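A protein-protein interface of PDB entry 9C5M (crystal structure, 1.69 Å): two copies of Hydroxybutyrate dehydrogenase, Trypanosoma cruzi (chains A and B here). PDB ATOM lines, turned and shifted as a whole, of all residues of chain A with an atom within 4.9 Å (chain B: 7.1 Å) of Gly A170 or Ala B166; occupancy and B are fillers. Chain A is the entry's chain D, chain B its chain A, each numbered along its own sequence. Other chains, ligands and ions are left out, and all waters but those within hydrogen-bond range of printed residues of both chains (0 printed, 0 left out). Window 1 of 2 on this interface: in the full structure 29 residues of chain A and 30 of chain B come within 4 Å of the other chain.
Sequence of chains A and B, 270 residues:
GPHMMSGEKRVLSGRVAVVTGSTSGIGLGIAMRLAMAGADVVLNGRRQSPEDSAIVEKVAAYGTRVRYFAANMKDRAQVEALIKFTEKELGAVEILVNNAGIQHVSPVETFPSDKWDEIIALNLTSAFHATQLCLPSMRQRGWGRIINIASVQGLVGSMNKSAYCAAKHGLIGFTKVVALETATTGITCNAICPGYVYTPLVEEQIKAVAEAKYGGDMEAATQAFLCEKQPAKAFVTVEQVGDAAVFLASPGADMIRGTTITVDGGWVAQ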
ATOM      1  N   LEU A 124      12.821 -36.043 -25.662  1.00  0.00           N
ATOM      2  CA  LEU A 124      13.730 -35.018 -25.153  1.00  0.00           C
ATOM      3  C   LEU A 124      13.560 -34.737 -23.666  1.00  0.00           C
ATOM      4  O   LEU A 124      14.500 -34.930 -22.890  1.00  0.00           O
ATOM      5  CB  LEU A 124      13.529 -33.721 -25.956  1.00  0.00           C
ATOM      6  CG  LEU A 124      14.257 -32.472 -25.454  1.00  0.00           C
ATOM      7  CD1 LEU A 124      15.748 -32.784 -25.284  1.00  0.00           C
ATOM      8  CD2 LEU A 124      14.036 -31.291 -26.379  1.00  0.00           C
ATOM      9  N   CYS A 165      12.952 -35.354 -35.489  1.00  0.00           N
ATOM     10  CA  CYS A 165      14.230 -34.704 -35.742  1.00  0.00           C
ATOM     11  C   CYS A 165      14.463 -33.568 -34.762  1.00  0.00           C
ATOM     12  O   CYS A 165      15.585 -33.369 -34.290  1.00  0.00           O
ATOM     13  CB  CYS A 165      14.295 -34.190 -37.175  1.00  0.00           C
ATOM     14  SG  CYS A 165      14.412 -35.543 -38.374  1.00  0.00           S
ATOM     15  N   ALA A 166      13.424 -32.789 -34.467  1.00  0.00           N
ATOM     16  CA  ALA A 166      13.589 -31.711 -33.501  1.00  0.00           C
ATOM     17  C   ALA A 166      13.981 -32.265 -32.134  1.00  0.00           C
ATOM     18  O   ALA A 166      14.920 -31.778 -31.492  1.00  0.00           O
ATOM     19  CB  ALA A 166      12.301 -30.896 -33.410  1.00  0.00           C
ATOM     20  N   ALA A 167      13.271 -33.296 -31.679  1.00  0.00           N
ATOM     21  CA  ALA A 167      13.538 -33.846 -30.356  1.00  0.00           C
ATOM     22  C   ALA A 167      14.932 -34.463 -30.289  1.00  0.00           C
ATOM     23  O   ALA A 167      15.646 -34.280 -29.300  1.00  0.00           O
ATOM     24  CB  ALA A 167      12.453 -34.860 -29.991  1.00  0.00           C
ATOM     25  N   LYS A 168      15.358 -35.162 -31.346  1.00  0.00           N
ATOM     26  CA  LYS A 168      16.665 -35.818 -31.317  1.00  0.00           C
ATOM     27  C   LYS A 168      17.814 -34.811 -31.438  1.00  0.00           C
ATOM     28  O   LYS A 168      18.841 -34.951 -30.750  1.00  0.00           O
ATOM     29  CB  LYS A 168      16.733 -36.879 -32.413  1.00  0.00           C
ATOM     30  CG  LYS A 168      15.803 -38.072 -32.182  1.00  0.00           C
ATOM     31  CD  LYS A 168      16.118 -38.831 -30.889  1.00  0.00           C
ATOM     32  CE  LYS A 168      15.511 -40.226 -30.938  1.00  0.00           C
ATOM     33  NZ  LYS A 168      15.693 -40.988 -29.683  1.00  0.00           N
ATOM     34  N   HIS A 169      17.656 -33.778 -32.279  1.00  0.00           N
ATOM     35  CA  HIS A 169      18.608 -32.669 -32.266  1.00  0.00           C
ATOM     36  C   HIS A 169      18.703 -32.059 -30.865  1.00  0.00           C
ATOM     37  O   HIS A 169      19.801 -31.809 -30.347  1.00  0.00           O
ATOM     38  CB  HIS A 169      18.192 -31.584 -33.279  1.00  0.00           C
ATOM     39  CG  HIS A 169      18.637 -31.825 -34.695  1.00  0.00           C
ATOM     40  ND1 HIS A 169      18.155 -32.857 -35.471  1.00  0.00           N
ATOM     41  CD2 HIS A 169      19.477 -31.121 -35.492  1.00  0.00           C
ATOM     42  CE1 HIS A 169      18.694 -32.795 -36.676  1.00  0.00           C
ATOM     43  NE2 HIS A 169      19.510 -31.756 -36.712  1.00  0.00           N
ATOM     44  N   GLY A 170      17.548 -31.794 -30.240  1.00  0.00           N
ATOM     45  CA  GLY A 170      17.555 -31.213 -28.906  1.00  0.00           C
ATOM     46  C   GLY A 170      18.221 -32.113 -27.887  1.00  0.00           C
ATOM     47  O   GLY A 170      18.896 -31.642 -26.972  1.00  0.00           O
ATOM     48  N   LEU A 171      18.035 -33.420 -28.019  1.00  0.00           N
ATOM     49  CA  LEU A 171      18.691 -34.332 -27.096  1.00  0.00           C
ATOM     50  C   LEU A 171      20.204 -34.263 -27.245  1.00  0.00           C
ATOM     51  O   LEU A 171      20.938 -34.389 -26.250  1.00  0.00           O
ATOM     52  CB  LEU A 171      18.184 -35.751 -27.335  1.00  0.00           C
ATOM     53  CG  LEU A 171      18.728 -36.825 -26.392  1.00  0.00           C
ATOM     54  CD1 LEU A 171      18.324 -36.589 -24.941  1.00  0.00           C
ATOM     55  CD2 LEU A 171      18.232 -38.192 -26.875  1.00  0.00           C
ATOM     56  N   ILE A 172      20.691 -34.061 -28.467  1.00  0.00           N
ATOM     57  CA  ILE A 172      22.132 -33.897 -28.644  1.00  0.00           C
ATOM     58  C   ILE A 172      22.617 -32.594 -28.006  1.00  0.00           C
ATOM     59  O   ILE A 172      23.658 -32.562 -27.329  1.00  0.00           O
ATOM     60  CB  ILE A 172      22.474 -34.001 -30.143  1.00  0.00           C
ATOM     61  CG1 ILE A 172      22.270 -35.459 -30.589  1.00  0.00           C
ATOM     62  CG2 ILE A 172      23.880 -33.563 -30.411  1.00  0.00           C
ATOM     63  CD1 ILE A 172      22.440 -35.708 -32.069  1.00  0.00           C
ATOM     64  N   GLY A 173      21.862 -31.511 -28.179  1.00  0.00           N
ATOM     65  CA  GLY A 173      22.261 -30.261 -27.533  1.00  0.00           C
ATOM     66  C   GLY A 173      22.292 -30.372 -26.015  1.00  0.00           C
ATOM     67  O   GLY A 173      23.218 -29.872 -25.345  1.00  0.00           O
ATOM     68  N   PHE A 174      21.283 -31.044 -25.453  1.00  0.00           N
ATOM     69  CA  PHE A 174      21.246 -31.321 -24.022  1.00  0.00           C
ATOM     70  C   PHE A 174      22.484 -32.091 -23.582  1.00  0.00           C
ATOM     71  O   PHE A 174      23.091 -31.791 -22.542  1.00  0.00           O
ATOM     72  CB  PHE A 174      19.977 -32.117 -23.692  1.00  0.00           C
ATOM     73  CG  PHE A 174      19.844 -32.473 -22.232  1.00  0.00           C
ATOM     74  CD1 PHE A 174      19.606 -31.481 -21.296  1.00  0.00           C
ATOM     75  CD2 PHE A 174      19.963 -33.780 -21.790  1.00  0.00           C
ATOM     76  CE1 PHE A 174      19.489 -31.782 -19.949  1.00  0.00           C
ATOM     77  CE2 PHE A 174      19.839 -34.083 -20.442  1.00  0.00           C
ATOM     78  CZ  PHE A 174      19.618 -33.081 -19.522  1.00  0.00           C
ATOM     79  N   TRP B 116      12.039 -25.039 -18.016  1.00  0.00           N
ATOM     80  CA  TRP B 116      12.393 -25.911 -19.129  1.00  0.00           C
ATOM     81  C   TRP B 116      11.233 -26.009 -20.109  1.00  0.00           C
ATOM     82  O   TRP B 116      11.406 -25.852 -21.330  1.00  0.00           O
ATOM     83  CB  TRP B 116      12.783 -27.302 -18.610  1.00  0.00           C
ATOM     84  CG  TRP B 116      12.973 -28.312 -19.716  1.00  0.00           C
ATOM     85  CD1 TRP B 116      11.991 -28.953 -20.423  1.00  0.00           C
ATOM     86  CD2 TRP B 116      14.218 -28.793 -20.243  1.00  0.00           C
ATOM     87  NE1 TRP B 116      12.547 -29.797 -21.348  1.00  0.00           N
ATOM     88  CE2 TRP B 116      13.910 -29.718 -21.263  1.00  0.00           C
ATOM     89  CE3 TRP B 116      15.559 -28.537 -19.950  1.00  0.00           C
ATOM     90  CZ2 TRP B 116      14.891 -30.375 -21.996  1.00  0.00           C
ATOM     91  CZ3 TRP B 116      16.533 -29.199 -20.677  1.00  0.00           C
ATOM     92  CH2 TRP B 116      16.194 -30.103 -21.688  1.00  0.00           C
ATOM     93  N   ILE B 119      10.704 -22.770 -22.078  1.00  0.00           N
ATOM     94  CA  ILE B 119      11.710 -22.544 -23.108  1.00  0.00           C
ATOM     95  C   ILE B 119      11.480 -23.461 -24.302  1.00  0.00           C
ATOM     96  O   ILE B 119      11.615 -23.035 -25.454  1.00  0.00           O
ATOM     97  CB  ILE B 119      13.117 -22.711 -22.509  1.00  0.00           C
ATOM     98  CG1 ILE B 119      13.453 -21.484 -21.656  1.00  0.00           C
ATOM     99  CG2 ILE B 119      14.149 -22.869 -23.600  1.00  0.00           C
ATOM    100  CD1 ILE B 119      14.632 -21.680 -20.760  1.00  0.00           C
ATOM    101  N   ILE B 120      11.125 -24.725 -24.059  1.00  0.00           N
ATOM    102  CA  ILE B 120      10.800 -25.602 -25.181  1.00  0.00           C
ATOM    103  C   ILE B 120       9.584 -25.070 -25.929  1.00  0.00           C
ATOM    104  O   ILE B 120       9.573 -25.001 -27.166  1.00  0.00           O
ATOM    105  CB  ILE B 120      10.567 -27.045 -24.701  1.00  0.00           C
ATOM    106  CG1 ILE B 120      11.827 -27.610 -24.055  1.00  0.00           C
ATOM    107  CG2 ILE B 120      10.128 -27.918 -25.872  1.00  0.00           C
ATOM    108  CD1 ILE B 120      13.040 -27.578 -24.928  1.00  0.00           C
ATOM    109  N   LEU B 124      10.992 -23.519 -29.402  1.00  0.00           N
ATOM    110  CA  LEU B 124      10.899 -24.551 -30.427  1.00  0.00           C
ATOM    111  C   LEU B 124       9.473 -24.793 -30.929  1.00  0.00           C
ATOM    112  O   LEU B 124       9.200 -24.650 -32.118  1.00  0.00           O
ATOM    113  CB  LEU B 124      11.521 -25.851 -29.898  1.00  0.00           C
ATOM    114  CG  LEU B 124      11.265 -27.119 -30.709  1.00  0.00           C
ATOM    115  CD1 LEU B 124      11.798 -26.967 -32.128  1.00  0.00           C
ATOM    116  CD2 LEU B 124      11.892 -28.297 -30.009  1.00  0.00           C
ATOM    117  N   GLN B 153      23.983 -21.545 -29.904  1.00  0.00           N
ATOM    118  CA  GLN B 153      23.588 -22.539 -28.911  1.00  0.00           C
ATOM    119  C   GLN B 153      22.739 -23.655 -29.510  1.00  0.00           C
ATOM    120  O   GLN B 153      22.349 -24.582 -28.786  1.00  0.00           O
ATOM    121  CB  GLN B 153      22.813 -21.870 -27.773  1.00  0.00           C
ATOM    122  CG  GLN B 153      23.472 -20.634 -27.164  1.00  0.00           C
ATOM    123  CD  GLN B 153      24.679 -20.946 -26.312  1.00  0.00           C
ATOM    124  OE1 GLN B 153      25.217 -22.055 -26.352  1.00  0.00           O
ATOM    125  NE2 GLN B 153      25.114 -19.958 -25.526  1.00  0.00           N
ATOM    126  N   GLY B 154      22.426 -23.563 -30.803  1.00  0.00           N
ATOM    127  CA  GLY B 154      21.813 -24.644 -31.549  1.00  0.00           C
ATOM    128  C   GLY B 154      22.806 -25.539 -32.250  1.00  0.00           C
ATOM    129  O   GLY B 154      22.428 -26.559 -32.835  1.00  0.00           O
ATOM    130  N   LYS B 161      22.819 -23.710 -19.694  1.00  0.00           N
ATOM    131  CA  LYS B 161      21.784 -23.350 -20.667  1.00  0.00           C
ATOM    132  C   LYS B 161      21.204 -24.592 -21.323  1.00  0.00           C
ATOM    133  O   LYS B 161      20.999 -24.644 -22.535  1.00  0.00           O
ATOM    134  CB  LYS B 161      22.368 -22.391 -21.702  1.00  0.00           C
ATOM    135  CG  LYS B 161      22.839 -21.083 -21.081  1.00  0.00           C
ATOM    136  CD  LYS B 161      23.387 -20.123 -22.120  1.00  0.00           C
ATOM    137  CE  LYS B 161      23.569 -18.736 -21.513  1.00  0.00           C
ATOM    138  NZ  LYS B 161      24.249 -17.784 -22.429  1.00  0.00           N
ATOM    139  N   SER B 162      20.886 -25.610 -20.515  1.00  0.00           N
ATOM    140  CA  SER B 162      20.486 -26.899 -21.078  1.00  0.00           C
ATOM    141  C   SER B 162      19.188 -26.790 -21.874  1.00  0.00           C
ATOM    142  O   SER B 162      19.095 -27.294 -22.998  1.00  0.00           O
ATOM    143  CB  SER B 162      20.360 -27.951 -19.973  1.00  0.00           C
ATOM    144  OG  SER B 162      19.496 -27.552 -18.929  1.00  0.00           O
ATOM    145  N   ALA B 163      18.166 -26.143 -21.300  1.00  0.00           N
ATOM    146  CA  ALA B 163      16.884 -26.032 -21.990  1.00  0.00           C
ATOM    147  C   ALA B 163      17.023 -25.241 -23.282  1.00  0.00           C
ATOM    148  O   ALA B 163      16.485 -25.635 -24.324  1.00  0.00           O
ATOM    149  CB  ALA B 163      15.851 -25.370 -21.079  1.00  0.00           C
ATOM    150  N   TYR B 164      17.744 -24.126 -23.228  1.00  0.00           N
ATOM    151  CA  TYR B 164      17.907 -23.259 -24.387  1.00  0.00           C
ATOM    152  C   TYR B 164      18.708 -23.948 -25.483  1.00  0.00           C
ATOM    153  O   TYR B 164      18.307 -23.924 -26.654  1.00  0.00           O
ATOM    154  CB  TYR B 164      18.564 -21.965 -23.913  1.00  0.00           C
ATOM    155  CG  TYR B 164      18.742 -20.856 -24.913  1.00  0.00           C
ATOM    156  CD1 TYR B 164      19.874 -20.797 -25.722  1.00  0.00           C
ATOM    157  CD2 TYR B 164      17.821 -19.813 -24.992  1.00  0.00           C
ATOM    158  CE1 TYR B 164      20.059 -19.736 -26.613  1.00  0.00           C
ATOM    159  CE2 TYR B 164      17.992 -18.770 -25.873  1.00  0.00           C
ATOM    160  CZ  TYR B 164      19.109 -18.726 -26.675  1.00  0.00           C
ATOM    161  OH  TYR B 164      19.250 -17.662 -27.543  1.00  0.00           O
ATOM    162  N   CYS B 165      19.821 -24.600 -25.129  1.00  0.00           N
ATOM    163  CA  CYS B 165      20.578 -25.321 -26.148  1.00  0.00           C
ATOM    164  C   CYS B 165      19.739 -26.435 -26.755  1.00  0.00           C
ATOM    165  O   CYS B 165      19.807 -26.678 -27.963  1.00  0.00           O
ATOM    166  CB  CYS B 165      21.865 -25.898 -25.572  1.00  0.00           C
ATOM    167  SG  CYS B 165      23.110 -24.653 -25.156  1.00  0.00           S
ATOM    168  N   ALA B 166      18.957 -27.135 -25.930  1.00  0.00           N
ATOM    169  CA  ALA B 166      18.096 -28.191 -26.451  1.00  0.00           C
ATOM    170  C   ALA B 166      17.063 -27.627 -27.424  1.00  0.00           C
ATOM    171  O   ALA B 166      16.882 -28.149 -28.530  1.00  0.00           O
ATOM    172  CB  ALA B 166      17.411 -28.920 -25.293  1.00  0.00           C
ATOM    173  N   ALA B 167      16.394 -26.540 -27.040  1.00  0.00           N
ATOM    174  CA  ALA B 167      15.389 -25.947 -27.914  1.00  0.00           C
ATOM    175  C   ALA B 167      16.004 -25.441 -29.212  1.00  0.00           C
ATOM    176  O   ALA B 167      15.421 -25.600 -30.288  1.00  0.00           O
ATOM    177  CB  ALA B 167      14.672 -24.798 -27.202  1.00  0.00           C
ATOM    178  N   LYS B 168      17.167 -24.792 -29.132  1.00  0.00           N
ATOM    179  CA  LYS B 168      17.775 -24.218 -30.330  1.00  0.00           C
ATOM    180  C   LYS B 168      18.313 -25.305 -31.261  1.00  0.00           C
ATOM    181  O   LYS B 168      18.180 -25.205 -32.495  1.00  0.00           O
ATOM    182  CB  LYS B 168      18.881 -23.242 -29.927  1.00  0.00           C
ATOM    183  CG  LYS B 168      18.377 -21.972 -29.237  1.00  0.00           C
ATOM    184  CD  LYS B 168      17.424 -21.177 -30.113  1.00  0.00           C
ATOM    185  CE  LYS B 168      17.166 -19.777 -29.534  1.00  0.00           C
ATOM    186  NZ  LYS B 168      16.191 -18.978 -30.332  1.00  0.00           N
ATOM    187  N   HIS B 169      18.923 -26.352 -30.695  1.00  0.00           N
ATOM    188  CA  HIS B 169      19.280 -27.517 -31.498  1.00  0.00           C
ATOM    189  C   HIS B 169      18.034 -28.072 -32.182  1.00  0.00           C
ATOM    190  O   HIS B 169      18.034 -28.359 -33.390  1.00  0.00           O
ATOM    191  CB  HIS B 169      19.938 -28.595 -30.613  1.00  0.00           C
ATOM    192  CG  HIS B 169      21.428 -28.448 -30.442  1.00  0.00           C
ATOM    193  ND1 HIS B 169      22.000 -27.428 -29.710  1.00  0.00           N
ATOM    194  CD2 HIS B 169      22.455 -29.230 -30.858  1.00  0.00           C
ATOM    195  CE1 HIS B 169      23.316 -27.561 -29.723  1.00  0.00           C
ATOM    196  NE2 HIS B 169      23.617 -28.654 -30.398  1.00  0.00           N
ATOM    197  N   GLY B 170      16.944 -28.202 -31.423  1.00  0.00           N
ATOM    198  CA  GLY B 170      15.718 -28.726 -31.998  1.00  0.00           C
ATOM    199  C   GLY B 170      15.176 -27.864 -33.120  1.00  0.00           C
ATOM    200  O   GLY B 170      14.657 -28.379 -34.112  1.00  0.00           O
ATOM    201  N   LEU B 171      15.249 -26.540 -32.960  1.00  0.00           N
ATOM    202  CA  LEU B 171      14.769 -25.625 -33.992  1.00  0.00           C
ATOM    203  C   LEU B 171      15.568 -25.783 -35.278  1.00  0.00           C
ATOM    204  O   LEU B 171      15.007 -25.676 -36.379  1.00  0.00           O
ATOM    205  CB  LEU B 171      14.853 -24.183 -33.483  1.00  0.00           C
ATOM    206  CG  LEU B 171      14.291 -23.066 -34.362  1.00  0.00           C
ATOM    207  CD1 LEU B 171      12.833 -23.327 -34.610  1.00  0.00           C
ATOM    208  CD2 LEU B 171      14.501 -21.700 -33.701  1.00  0.00           C
ATOM    209  N   ILE B 172      16.866 -26.073 -35.159  1.00  0.00           N
ATOM    210  CA  ILE B 172      17.667 -26.323 -36.359  1.00  0.00           C
ATOM    211  C   ILE B 172      17.267 -27.646 -37.018  1.00  0.00           C
ATOM    212  O   ILE B 172      17.155 -27.740 -38.254  1.00  0.00           O
ATOM    213  CB  ILE B 172      19.166 -26.267 -36.001  1.00  0.00           C
ATOM    214  CG1 ILE B 172      19.564 -24.828 -35.623  1.00  0.00           C
ATOM    215  CG2 ILE B 172      20.037 -26.741 -37.153  1.00  0.00           C
ATOM    216  CD1 ILE B 172      20.989 -24.676 -35.148  1.00  0.00           C
ATOM    217  N   GLY B 173      17.027 -28.690 -36.220  1.00  0.00           N
ATOM    218  CA  GLY B 173      16.545 -29.938 -36.808  1.00  0.00           C
ATOM    219  C   GLY B 173      15.209 -29.766 -37.516  1.00  0.00           C
ATOM    220  O   GLY B 173      14.991 -30.284 -38.627  1.00  0.00           O
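O of Gly B154 sits close to ND1 of His B169.
O of Cys B165 sits at hydrogen-bond distance from ND1 of His B169, 2.9 Å away.
A ring nitrogen (ND1) of His A169 lies within hydrogen-bond range of the backbone carbonyl oxygen (O) of Cys A165, 2.9 Å away.
The backbone carbonyl oxygen of Gln B153 sits at hydrogen-bond distance from a ring nitrogen (ND1) of His B169 (3.0 Å).
Among the printed residues, pairs that only touch across the chains: Gly A170 with Ala B166, Ala A166 with Gly B170, His A169 with His B169, His A169 with Gly B173, Gly A173 with His B169, Phe A174 with Trp B116, Gly A170 with Gly B170, Phe A174 with Ser B162, Gly A170 with His B169 and His A169 with Gly B170.
Of the printed residues of chain B, Gly A170 touches Ala B166 (3.2 Å), His B169 (3.9 Å) and Gly B170 (3.8 Å).
Of the printed residues of chain B, Gly A173 touches His B169.
Printed residues of chain B within 4 Å of Phe A174: Trp B116 and Ser B162.
Of the printed residues of chain A, Ser B162 touches Phe A174 (3.8 Å).
Ala B166 touches just one residue of chain A: Gly A170.
Of the printed residues of chain A, Gly B173 touches His A169 (3.4 Å).
The nearest printed residue of chain B that does not touch Gly A170 is Cys B165 (5.1 Å).
The nearest printed residue of chain A that does not touch Gly B173 is Cys A165 (4.2 Å).
Hydrophobic or aromatic side chains of chain A within 4 Å of the printed part of chain B: Ala A166, His A169 and Phe A174.
Of the 19 printed residues of chain B, 6 touch a printed residue of chain A.
Printed residues of chain B that touch a printed residue of chain A: Trp B116, Ser B162, Ala B166, His B169, Gly B170 and Gly B173.
Hydrophobic or aromatic side chains of chain B within 4 Å of the printed part of chain A: Trp B116, Ala B166 and His B169.
Among the printed residues, 10 pairs touch across the chains.
Among the printed residues, no Asp or Glu carboxylate lies within 4 Å of a Lys or Arg side-chain nitrogen of the other chain.
Ala A166 touches Gly B170, and with the chains exchanged Gly A170 touches Ala B166.
His A169 touches its own counterpart, His B169.
His A169 touches Gly B170, and with the chains exchanged Gly A170 touches His B169.
Gly A170 touches its own counterpart, Gly B170.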
